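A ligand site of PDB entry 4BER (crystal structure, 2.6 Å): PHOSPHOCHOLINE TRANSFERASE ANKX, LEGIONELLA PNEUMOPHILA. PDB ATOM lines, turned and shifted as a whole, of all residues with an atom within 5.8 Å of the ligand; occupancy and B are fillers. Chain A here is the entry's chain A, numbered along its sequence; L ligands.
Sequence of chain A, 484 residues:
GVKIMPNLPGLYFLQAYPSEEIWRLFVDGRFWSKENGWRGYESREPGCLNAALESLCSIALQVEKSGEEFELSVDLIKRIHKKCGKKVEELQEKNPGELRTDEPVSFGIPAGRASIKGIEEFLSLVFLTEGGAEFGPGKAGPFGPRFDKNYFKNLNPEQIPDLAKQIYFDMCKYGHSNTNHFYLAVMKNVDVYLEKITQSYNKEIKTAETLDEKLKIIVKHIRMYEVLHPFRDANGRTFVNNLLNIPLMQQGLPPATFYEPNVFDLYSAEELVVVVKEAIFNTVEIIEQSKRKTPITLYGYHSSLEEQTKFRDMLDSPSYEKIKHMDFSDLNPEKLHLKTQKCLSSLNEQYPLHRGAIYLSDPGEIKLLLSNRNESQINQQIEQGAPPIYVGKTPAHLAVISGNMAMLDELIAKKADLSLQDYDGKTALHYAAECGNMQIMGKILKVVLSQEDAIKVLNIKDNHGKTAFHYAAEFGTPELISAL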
ATOM      1  N   PHE A  26     -32.331  10.925   4.272  1.00  0.00           N
ATOM      2  CA  PHE A  26     -30.924  10.578   3.981  1.00  0.00           C
ATOM      3  C   PHE A  26     -30.716   9.070   3.846  1.00  0.00           C
ATOM      4  O   PHE A  26     -29.946   8.634   2.961  1.00  0.00           O
ATOM      5  CB  PHE A  26     -29.950  11.205   5.016  1.00  0.00           C
ATOM      6  CG  PHE A  26     -30.156  12.690   5.140  1.00  0.00           C
ATOM      7  CD1 PHE A  26     -29.706  13.563   4.148  1.00  0.00           C
ATOM      8  CD2 PHE A  26     -30.914  13.221   6.188  1.00  0.00           C
ATOM      9  CE1 PHE A  26     -29.966  14.942   4.227  1.00  0.00           C
ATOM     10  CE2 PHE A  26     -31.182  14.588   6.254  1.00  0.00           C
ATOM     11  CZ  PHE A  26     -30.708  15.449   5.273  1.00  0.00           C
ATOM     12  N   ASP A  28     -31.590   5.707   2.620  1.00  0.00           N
ATOM     13  CA  ASP A  28     -32.314   5.089   1.492  1.00  0.00           C
ATOM     14  C   ASP A  28     -33.412   4.177   2.020  1.00  0.00           C
ATOM     15  O   ASP A  28     -33.113   3.352   2.871  1.00  0.00           O
ATOM     16  CB  ASP A  28     -31.373   4.227   0.632  1.00  0.00           C
ATOM     17  CG  ASP A  28     -30.034   4.788   0.228  1.00  0.00           C
ATOM     18  OD1 ASP A  28     -29.699   5.913   0.668  1.00  0.00           O
ATOM     19  OD2 ASP A  28     -29.315   4.105  -0.545  1.00  0.00           O
ATOM     20  N   ARG A  30     -34.600   1.576   0.909  1.00  0.00           N
ATOM     21  CA  ARG A  30     -34.175   0.187   0.701  1.00  0.00           C
ATOM     22  C   ARG A  30     -33.548  -0.481   1.933  1.00  0.00           C
ATOM     23  O   ARG A  30     -33.548  -1.715   2.030  1.00  0.00           O
ATOM     24  CB  ARG A  30     -33.254   0.080  -0.524  1.00  0.00           C
ATOM     25  CG  ARG A  30     -31.885   0.713  -0.315  1.00  0.00           C
ATOM     26  CD  ARG A  30     -31.216   1.048  -1.608  1.00  0.00           C
ATOM     27  NE  ARG A  30     -29.823   1.474  -1.392  1.00  0.00           N
ATOM     28  CZ  ARG A  30     -28.776   0.652  -1.420  1.00  0.00           C
ATOM     29  NH1 ARG A  30     -28.951  -0.653  -1.623  1.00  0.00           N
ATOM     30  NH2 ARG A  30     -27.552   1.121  -1.232  1.00  0.00           N
ATOM     31  N   PHE A  31     -33.028   0.327   2.873  1.00  0.00           N
ATOM     32  CA  PHE A  31     -32.366  -0.132   4.104  1.00  0.00           C
ATOM     33  C   PHE A  31     -33.287  -0.373   5.276  1.00  0.00           C
ATOM     34  O   PHE A  31     -32.982  -1.213   6.123  1.00  0.00           O
ATOM     35  CB  PHE A  31     -31.316   0.892   4.559  1.00  0.00           C
ATOM     36  CG  PHE A  31     -30.165   1.170   3.625  1.00  0.00           C
ATOM     37  CD1 PHE A  31     -29.565   0.137   2.909  1.00  0.00           C
ATOM     38  CD2 PHE A  31     -29.630   2.449   3.511  1.00  0.00           C
ATOM     39  CE1 PHE A  31     -28.463   0.384   2.084  1.00  0.00           C
ATOM     40  CE2 PHE A  31     -28.548   2.700   2.664  1.00  0.00           C
ATOM     41  CZ  PHE A  31     -27.950   1.654   1.978  1.00  0.00           C
ATOM     42  N   GLY A  40     -28.390   0.985  10.677  1.00  0.00           N
ATOM     43  CA  GLY A  40     -27.363   0.465   9.788  1.00  0.00           C
ATOM     44  C   GLY A  40     -26.536   1.577   9.170  1.00  0.00           C
ATOM     45  O   GLY A  40     -25.294   1.570   9.282  1.00  0.00           O
ATOM     46  N   TYR A  41     -27.236   2.565   8.569  1.00  0.00           N
ATOM     47  CA  TYR A  41     -26.681   3.763   7.944  1.00  0.00           C
ATOM     48  C   TYR A  41     -25.757   4.530   8.917  1.00  0.00           C
ATOM     49  O   TYR A  41     -24.610   4.807   8.550  1.00  0.00           O
ATOM     50  CB  TYR A  41     -27.830   4.660   7.430  1.00  0.00           C
ATOM     51  CG  TYR A  41     -27.433   5.798   6.514  1.00  0.00           C
ATOM     52  CD1 TYR A  41     -26.941   7.000   7.024  1.00  0.00           C
ATOM     53  CD2 TYR A  41     -27.683   5.733   5.143  1.00  0.00           C
ATOM     54  CE1 TYR A  41     -26.608   8.059   6.183  1.00  0.00           C
ATOM     55  CE2 TYR A  41     -27.374   6.805   4.289  1.00  0.00           C
ATOM     56  CZ  TYR A  41     -26.836   7.968   4.824  1.00  0.00           C
ATOM     57  OH  TYR A  41     -26.543   9.052   4.031  1.00  0.00           O
ATOM     58  N   GLU A  42     -26.253   4.858  10.142  1.00  0.00           N
ATOM     59  CA  GLU A  42     -25.499   5.597  11.174  1.00  0.00           C
ATOM     60  C   GLU A  42     -24.213   4.886  11.599  1.00  0.00           C
ATOM     61  O   GLU A  42     -23.182   5.530  11.685  1.00  0.00           O
ATOM     62  CB  GLU A  42     -26.351   5.835  12.440  1.00  0.00           C
ATOM     63  CG  GLU A  42     -26.517   7.296  12.830  1.00  0.00           C
ATOM     64  CD  GLU A  42     -25.267   8.087  13.173  1.00  0.00           C
ATOM     65  OE1 GLU A  42     -24.547   7.704  14.133  1.00  0.00           O
ATOM     66  OE2 GLU A  42     -25.044   9.139  12.522  1.00  0.00           O
ATOM     67  N   ARG A  44     -22.362   2.752  10.019  1.00  0.00           N
ATOM     68  CA  ARG A  44     -21.423   2.738   8.892  1.00  0.00           C
ATOM     69  C   ARG A  44     -20.465   3.959   8.893  1.00  0.00           C
ATOM     70  O   ARG A  44     -19.298   3.812   8.507  1.00  0.00           O
ATOM     71  CB  ARG A  44     -22.212   2.694   7.597  1.00  0.00           C
ATOM     72  CG  ARG A  44     -21.767   1.623   6.614  1.00  0.00           C
ATOM     73  CD  ARG A  44     -22.802   1.528   5.500  1.00  0.00           C
ATOM     74  NE  ARG A  44     -23.912   0.673   5.914  1.00  0.00           N
ATOM     75  CZ  ARG A  44     -25.197   0.948   5.745  1.00  0.00           C
ATOM     76  NH1 ARG A  44     -25.573   2.070   5.158  1.00  0.00           N
ATOM     77  NH2 ARG A  44     -26.115   0.104   6.165  1.00  0.00           N
ATOM     78  N   GLU A  45     -20.973   5.146   9.298  1.00  0.00           N
ATOM     79  CA  GLU A  45     -20.242   6.418   9.394  1.00  0.00           C
ATOM     80  C   GLU A  45     -20.820   7.246  10.555  1.00  0.00           C
ATOM     81  O   GLU A  45     -21.641   8.122  10.303  1.00  0.00           O
ATOM     82  CB  GLU A  45     -20.321   7.221   8.077  1.00  0.00           C
ATOM     83  CG  GLU A  45     -19.420   6.709   6.965  1.00  0.00           C
ATOM     84  CD  GLU A  45     -19.670   7.236   5.571  1.00  0.00           C
ATOM     85  OE1 GLU A  45     -19.956   8.457   5.436  1.00  0.00           O
ATOM     86  OE2 GLU A  45     -19.541   6.449   4.611  1.00  0.00           O
ATOM     87  N   CYS A  48     -22.720  10.987  10.497  1.00  0.00           N
ATOM     88  CA  CYS A  48     -23.024  11.352   9.114  1.00  0.00           C
ATOM     89  C   CYS A  48     -24.458  11.868   8.937  1.00  0.00           C
ATOM     90  O   CYS A  48     -24.692  12.700   8.052  1.00  0.00           O
ATOM     91  CB  CYS A  48     -22.722  10.204   8.175  1.00  0.00           C
ATOM     92  SG  CYS A  48     -23.862   8.807   8.331  1.00  0.00           S
ATOM     93  N   ARG A 113     -29.712  -0.455 -11.399  1.00  0.00           N
ATOM     94  CA  ARG A 113     -29.469   0.994 -11.215  1.00  0.00           C
ATOM     95  C   ARG A 113     -29.232   1.709 -12.551  1.00  0.00           C
ATOM     96  O   ARG A 113     -28.821   2.879 -12.584  1.00  0.00           O
ATOM     97  CB  ARG A 113     -28.271   1.196 -10.268  1.00  0.00           C
ATOM     98  CG  ARG A 113     -28.657   1.073  -8.810  1.00  0.00           C
ATOM     99  CD  ARG A 113     -27.424   1.113  -7.957  1.00  0.00           C
ATOM    100  NE  ARG A 113     -27.722   1.036  -6.524  1.00  0.00           N
ATOM    101  CZ  ARG A 113     -26.796   1.165  -5.578  1.00  0.00           C
ATOM    102  NH1 ARG A 113     -25.522   1.380  -5.901  1.00  0.00           N
ATOM    103  NH2 ARG A 113     -27.129   1.077  -4.300  1.00  0.00           N
ATOM    104  N   GLU A 226     -23.351  14.228 -10.401  1.00  0.00           N
ATOM    105  CA  GLU A 226     -23.088  12.929  -9.780  1.00  0.00           C
ATOM    106  C   GLU A 226     -22.127  12.119 -10.675  1.00  0.00           C
ATOM    107  O   GLU A 226     -21.165  11.551 -10.171  1.00  0.00           O
ATOM    108  CB  GLU A 226     -24.420  12.204  -9.512  1.00  0.00           C
ATOM    109  CG  GLU A 226     -24.311  10.706  -9.230  1.00  0.00           C
ATOM    110  CD  GLU A 226     -23.345  10.230  -8.163  1.00  0.00           C
ATOM    111  OE1 GLU A 226     -23.219  10.906  -7.116  1.00  0.00           O
ATOM    112  OE2 GLU A 226     -22.711   9.172  -8.390  1.00  0.00           O
ATOM    113  N   HIS A 229     -17.712  12.819 -11.002  1.00  0.00           N
ATOM    114  CA  HIS A 229     -17.651  12.593  -9.557  1.00  0.00           C
ATOM    115  C   HIS A 229     -16.638  13.656  -9.054  1.00  0.00           C
ATOM    116  O   HIS A 229     -15.446  13.457  -9.248  1.00  0.00           O
ATOM    117  CB  HIS A 229     -17.224  11.135  -9.304  1.00  0.00           C
ATOM    118  CG  HIS A 229     -18.069  10.404  -8.325  1.00  0.00           C
ATOM    119  ND1 HIS A 229     -19.443  10.337  -8.449  1.00  0.00           N
ATOM    120  CD2 HIS A 229     -17.701   9.686  -7.235  1.00  0.00           C
ATOM    121  CE1 HIS A 229     -19.867   9.612  -7.419  1.00  0.00           C
ATOM    122  NE2 HIS A 229     -18.850   9.212  -6.666  1.00  0.00           N
ATOM    123  N   ASP A 233     -15.378  11.426  -1.937  1.00  0.00           N
ATOM    124  CA  ASP A 233     -16.596  10.740  -1.498  1.00  0.00           C
ATOM    125  C   ASP A 233     -17.668  11.784  -1.147  1.00  0.00           C
ATOM    126  O   ASP A 233     -17.455  12.978  -1.373  1.00  0.00           O
ATOM    127  CB  ASP A 233     -16.334   9.706  -0.363  1.00  0.00           C
ATOM    128  CG  ASP A 233     -17.427   8.639  -0.214  1.00  0.00           C
ATOM    129  OD1 ASP A 233     -17.453   7.671  -1.030  1.00  0.00           O
ATOM    130  OD2 ASP A 233     -18.261   8.778   0.702  1.00  0.00           O
ATOM    131  N   ALA A 234     -18.843  11.336  -0.651  1.00  0.00           N
ATOM    132  CA  ALA A 234     -20.006  12.125  -0.278  1.00  0.00           C
ATOM    133  C   ALA A 234     -20.720  12.843  -1.426  1.00  0.00           C
ATOM    134  O   ALA A 234     -21.497  13.758  -1.150  1.00  0.00           O
ATOM    135  CB  ALA A 234     -19.701  13.078   0.889  1.00  0.00           C
ATOM    136  N   ASN A 235     -20.557  12.375  -2.685  1.00  0.00           N
ATOM    137  CA  ASN A 235     -21.201  12.976  -3.868  1.00  0.00           C
ATOM    138  C   ASN A 235     -22.724  12.755  -3.895  1.00  0.00           C
ATOM    139  O   ASN A 235     -23.470  13.610  -4.378  1.00  0.00           O
ATOM    140  CB  ASN A 235     -20.587  12.476  -5.168  1.00  0.00           C
ATOM    141  CG  ASN A 235     -19.116  12.698  -5.265  1.00  0.00           C
ATOM    142  OD1 ASN A 235     -18.655  13.792  -5.613  1.00  0.00           O
ATOM    143  ND2 ASN A 235     -18.347  11.690  -4.908  1.00  0.00           N
ATOM    144  N   GLY A 236     -23.157  11.599  -3.425  1.00  0.00           N
ATOM    145  CA  GLY A 236     -24.572  11.279  -3.327  1.00  0.00           C
ATOM    146  C   GLY A 236     -25.242  12.224  -2.366  1.00  0.00           C
ATOM    147  O   GLY A 236     -26.180  12.927  -2.726  1.00  0.00           O
ATOM    148  N   ARG A 237     -24.729  12.288  -1.132  1.00  0.00           N
ATOM    149  CA  ARG A 237     -25.233  13.163  -0.083  1.00  0.00           C
ATOM    150  C   ARG A 237     -25.201  14.629  -0.485  1.00  0.00           C
ATOM    151  O   ARG A 237     -26.193  15.328  -0.288  1.00  0.00           O
ATOM    152  CB  ARG A 237     -24.473  12.953   1.223  1.00  0.00           C
ATOM    153  CG  ARG A 237     -24.995  11.772   1.996  1.00  0.00           C
ATOM    154  CD  ARG A 237     -24.026  11.390   3.076  1.00  0.00           C
ATOM    155  NE  ARG A 237     -22.939  10.590   2.527  1.00  0.00           N
ATOM    156  CZ  ARG A 237     -21.872  10.193   3.215  1.00  0.00           C
ATOM    157  NH1 ARG A 237     -21.744  10.534   4.492  1.00  0.00           N
ATOM    158  NH2 ARG A 237     -20.939   9.461   2.634  1.00  0.00           N
ATOM    159  N   THR A 238     -24.067  15.070  -1.073  1.00  0.00           N
ATOM    160  CA  THR A 238     -23.843  16.451  -1.528  1.00  0.00           C
ATOM    161  C   THR A 238     -24.869  16.832  -2.585  1.00  0.00           C
ATOM    162  O   THR A 238     -25.599  17.807  -2.385  1.00  0.00           O
ATOM    163  CB  THR A 238     -22.387  16.637  -2.035  1.00  0.00           C
ATOM    164  OG1 THR A 238     -21.470  16.395  -0.970  1.00  0.00           O
ATOM    165  CG2 THR A 238     -22.135  18.008  -2.655  1.00  0.00           C
ATOM    166  N   ASN A 241     -28.936  14.209  -1.871  1.00  0.00           N
ATOM    167  CA  ASN A 241     -29.591  14.385  -0.575  1.00  0.00           C
ATOM    168  C   ASN A 241     -29.630  15.835  -0.115  1.00  0.00           C
ATOM    169  O   ASN A 241     -30.484  16.179   0.699  1.00  0.00           O
ATOM    170  CB  ASN A 241     -28.981  13.455   0.463  1.00  0.00           C
ATOM    171  CG  ASN A 241     -29.232  12.012   0.153  1.00  0.00           C
ATOM    172  OD1 ASN A 241     -30.374  11.558   0.101  1.00  0.00           O
ATOM    173  ND2 ASN A 241     -28.164  11.273  -0.131  1.00  0.00           N
ATOM    174  N   GLU A 260     -34.270   4.410  -3.308  1.00  0.00           N
ATOM    175  CA  GLU A 260     -32.962   4.169  -3.941  1.00  0.00           C
ATOM    176  C   GLU A 260     -32.482   5.446  -4.706  1.00  0.00           C
ATOM    177  O   GLU A 260     -32.879   5.669  -5.869  1.00  0.00           O
ATOM    178  CB  GLU A 260     -33.043   2.936  -4.904  1.00  0.00           C
ATOM    179  CG  GLU A 260     -31.812   2.663  -5.753  1.00  0.00           C
ATOM    180  CD  GLU A 260     -30.524   2.379  -4.996  1.00  0.00           C
ATOM    181  OE1 GLU A 260     -29.911   3.345  -4.496  1.00  0.00           O
ATOM    182  OE2 GLU A 260     -30.124   1.190  -4.921  1.00  0.00           O
ATOM    183  N   PRO A 261     -31.652   6.247  -4.053  1.00  0.00           N
ATOM    184  CA  PRO A 261     -31.117   7.471  -4.660  1.00  0.00           C
ATOM    185  C   PRO A 261     -29.862   7.202  -5.481  1.00  0.00           C
ATOM    186  O   PRO A 261     -29.243   8.144  -5.979  1.00  0.00           O
ATOM    187  CB  PRO A 261     -30.792   8.341  -3.453  1.00  0.00           C
ATOM    188  CG  PRO A 261     -30.503   7.365  -2.362  1.00  0.00           C
ATOM    189  CD  PRO A 261     -31.417   6.201  -2.606  1.00  0.00           C
ATOM    190  N   ASN A 262     -29.487   5.934  -5.607  1.00  0.00           N
ATOM    191  CA  ASN A 262     -28.300   5.557  -6.353  1.00  0.00           C
ATOM    192  C   ASN A 262     -28.606   5.263  -7.815  1.00  0.00           C
ATOM    193  O   ASN A 262     -28.142   4.270  -8.373  1.00  0.00           O
ATOM    194  CB  ASN A 262     -27.625   4.330  -5.711  1.00  0.00           C
ATOM    195  CG  ASN A 262     -26.631   4.723  -4.639  1.00  0.00           C
ATOM    196  OD1 ASN A 262     -25.604   5.345  -4.919  1.00  0.00           O
ATOM    197  ND2 ASN A 262     -26.929   4.352  -3.393  1.00  0.00           N
HETATM  198  O1  LIG L   1     -21.510   9.407  -2.178  1.00  0.00           O
HETATM  199  P1  LIG L   1     -22.139   8.927  -0.873  1.00  0.00           P
HETATM  200  O2  LIG L   1     -21.170   8.156  -0.010  1.00  0.00           O
HETATM  201  O3  LIG L   1     -22.800  10.110  -0.146  1.00  0.00           O
HETATM  202  O4  LIG L   1     -23.354   8.017  -1.307  1.00  0.00           O
HETATM  203  C1  LIG L   1     -24.700   8.053  -0.786  1.00  0.00           C
HETATM  204  C2  LIG L   1     -25.228   6.657  -0.651  1.00  0.00           C
HETATM  205  O5  LIG L   1     -24.248   5.814   0.012  1.00  0.00           O
HETATM  206  C3  LIG L   1     -26.481   6.522   0.204  1.00  0.00           C
HETATM  207  O6  LIG L   1     -27.635   6.806  -0.577  1.00  0.00           O
HETATM  208  C4  LIG L   1     -26.391   5.083   0.672  1.00  0.00           C
HETATM  209  O7  LIG L   1     -26.739   4.143  -0.340  1.00  0.00           O
HETATM  210  C5  LIG L   1     -24.893   4.952   0.932  1.00  0.00           C
HETATM  211  N1  LIG L   1     -24.501   5.328   2.319  1.00  0.00           N
HETATM  212  C6  LIG L   1     -24.801   4.424   3.340  1.00  0.00           C
HETATM  213  N2  LIG L   1     -24.458   4.735   4.620  1.00  0.00           N
HETATM  214  C7  LIG L   1     -23.821   5.893   4.892  1.00  0.00           C
HETATM  215  C8  LIG L   1     -23.507   6.830   3.860  1.00  0.00           C
HETATM  216  C9  LIG L   1     -23.863   6.522   2.601  1.00  0.00           C
HETATM  217  O8  LIG L   1     -25.373   3.368   3.063  1.00  0.00           O
HETATM  218  N3  LIG L   1     -23.466   6.136   6.155  1.00  0.00           N
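The guanidinium group of Arg 30 is in salt-bridge range of the side-chain carboxylate of Glu 260.
NH1 of Arg 237 lies within salt-bridge range of OE1 of Glu 45, at 2.9 Å.
The side-chain carboxylate (OD2) of Asp 233 lies within salt-bridge range of the guanidinium group (NH2) of Arg 237, 3.4 Å away.
OD2 of Asp 28 lies within salt-bridge range of NE of Arg 30.
SG of Cys 48 sits at hydrogen-bond distance from O of Glu 45 (3.0 Å).
The side-chain amide nitrogen (ND2) of Asn 235 lies within hydrogen-bond range of a ring nitrogen (NE2) of His 229, at 3.1 Å.
The side-chain hydroxyl (OG1) of Thr 238 is in hydrogen-bond range of the backbone carbonyl oxygen (O) of Ala 234, 2.6 Å away.
The side-chain carboxylate (OE1) of Glu 260 lies close to the backbone NH (N) of Asn 262, 2.8 Å away.
CE2 of Phe 31 touches O8 of the ligand, at 3.3 Å.
Glu 45 touches the ligand.
Ala 234 touches the ligand (CA to O3, 3.4 Å).
Pro 261 touches the ligand (CG to O6, 3.4 Å).
Hydrophobic or aromatic side chains that line the ligand: Phe 31, Tyr 41 and Pro 261.
14 residues have an atom within 4 Å of the ligand: Asp 28, Arg 30, Phe 31, Tyr 41, Arg 44, Glu 45, Cys 48, Asp 233, Ala 234, Asn 235, Gly 236, Arg 237, Pro 261 and Asn 262.
N of Gly 236 sits at hydrogen-bond distance from O1 of the ligand.
An oxygen (O8) of the ligand sits at hydrogen-bond distance from the guanidinium group (NH1) of Arg 44 (2.5 Å).
NH2 of Arg 30 is in hydrogen-bond range of O7 of the ligand (3.3 Å).
N of Arg 237 is in hydrogen-bond range of O3 of the ligand.
The backbone carbonyl oxygen (O) of Tyr 41 is in hydrogen-bond range of a nitrogen (N3) of the ligand (3.0 Å).
The side-chain carboxylate (OD1) of Asp 28 is in hydrogen-bond range of an oxygen (O6) of the ligand.
SG of Cys 48 lies within hydrogen-bond range of N3 of the ligand, 3.5 Å away.
The side-chain carboxylate (OD2) of Asp 233 sits close to an oxygen (O2) of the ligand, 3.1 Å away.
An oxygen (O7) of the ligand lies within hydrogen-bond range of the side-chain amide nitrogen of Asn 262 (3.1 Å).
The backbone NH (N) of Asn 235 lies within hydrogen-bond range of an oxygen (O1) of the ligand (3.2 Å).
O3 of the ligand is in salt-bridge range of NE of Arg 237, 2.7 Å away.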
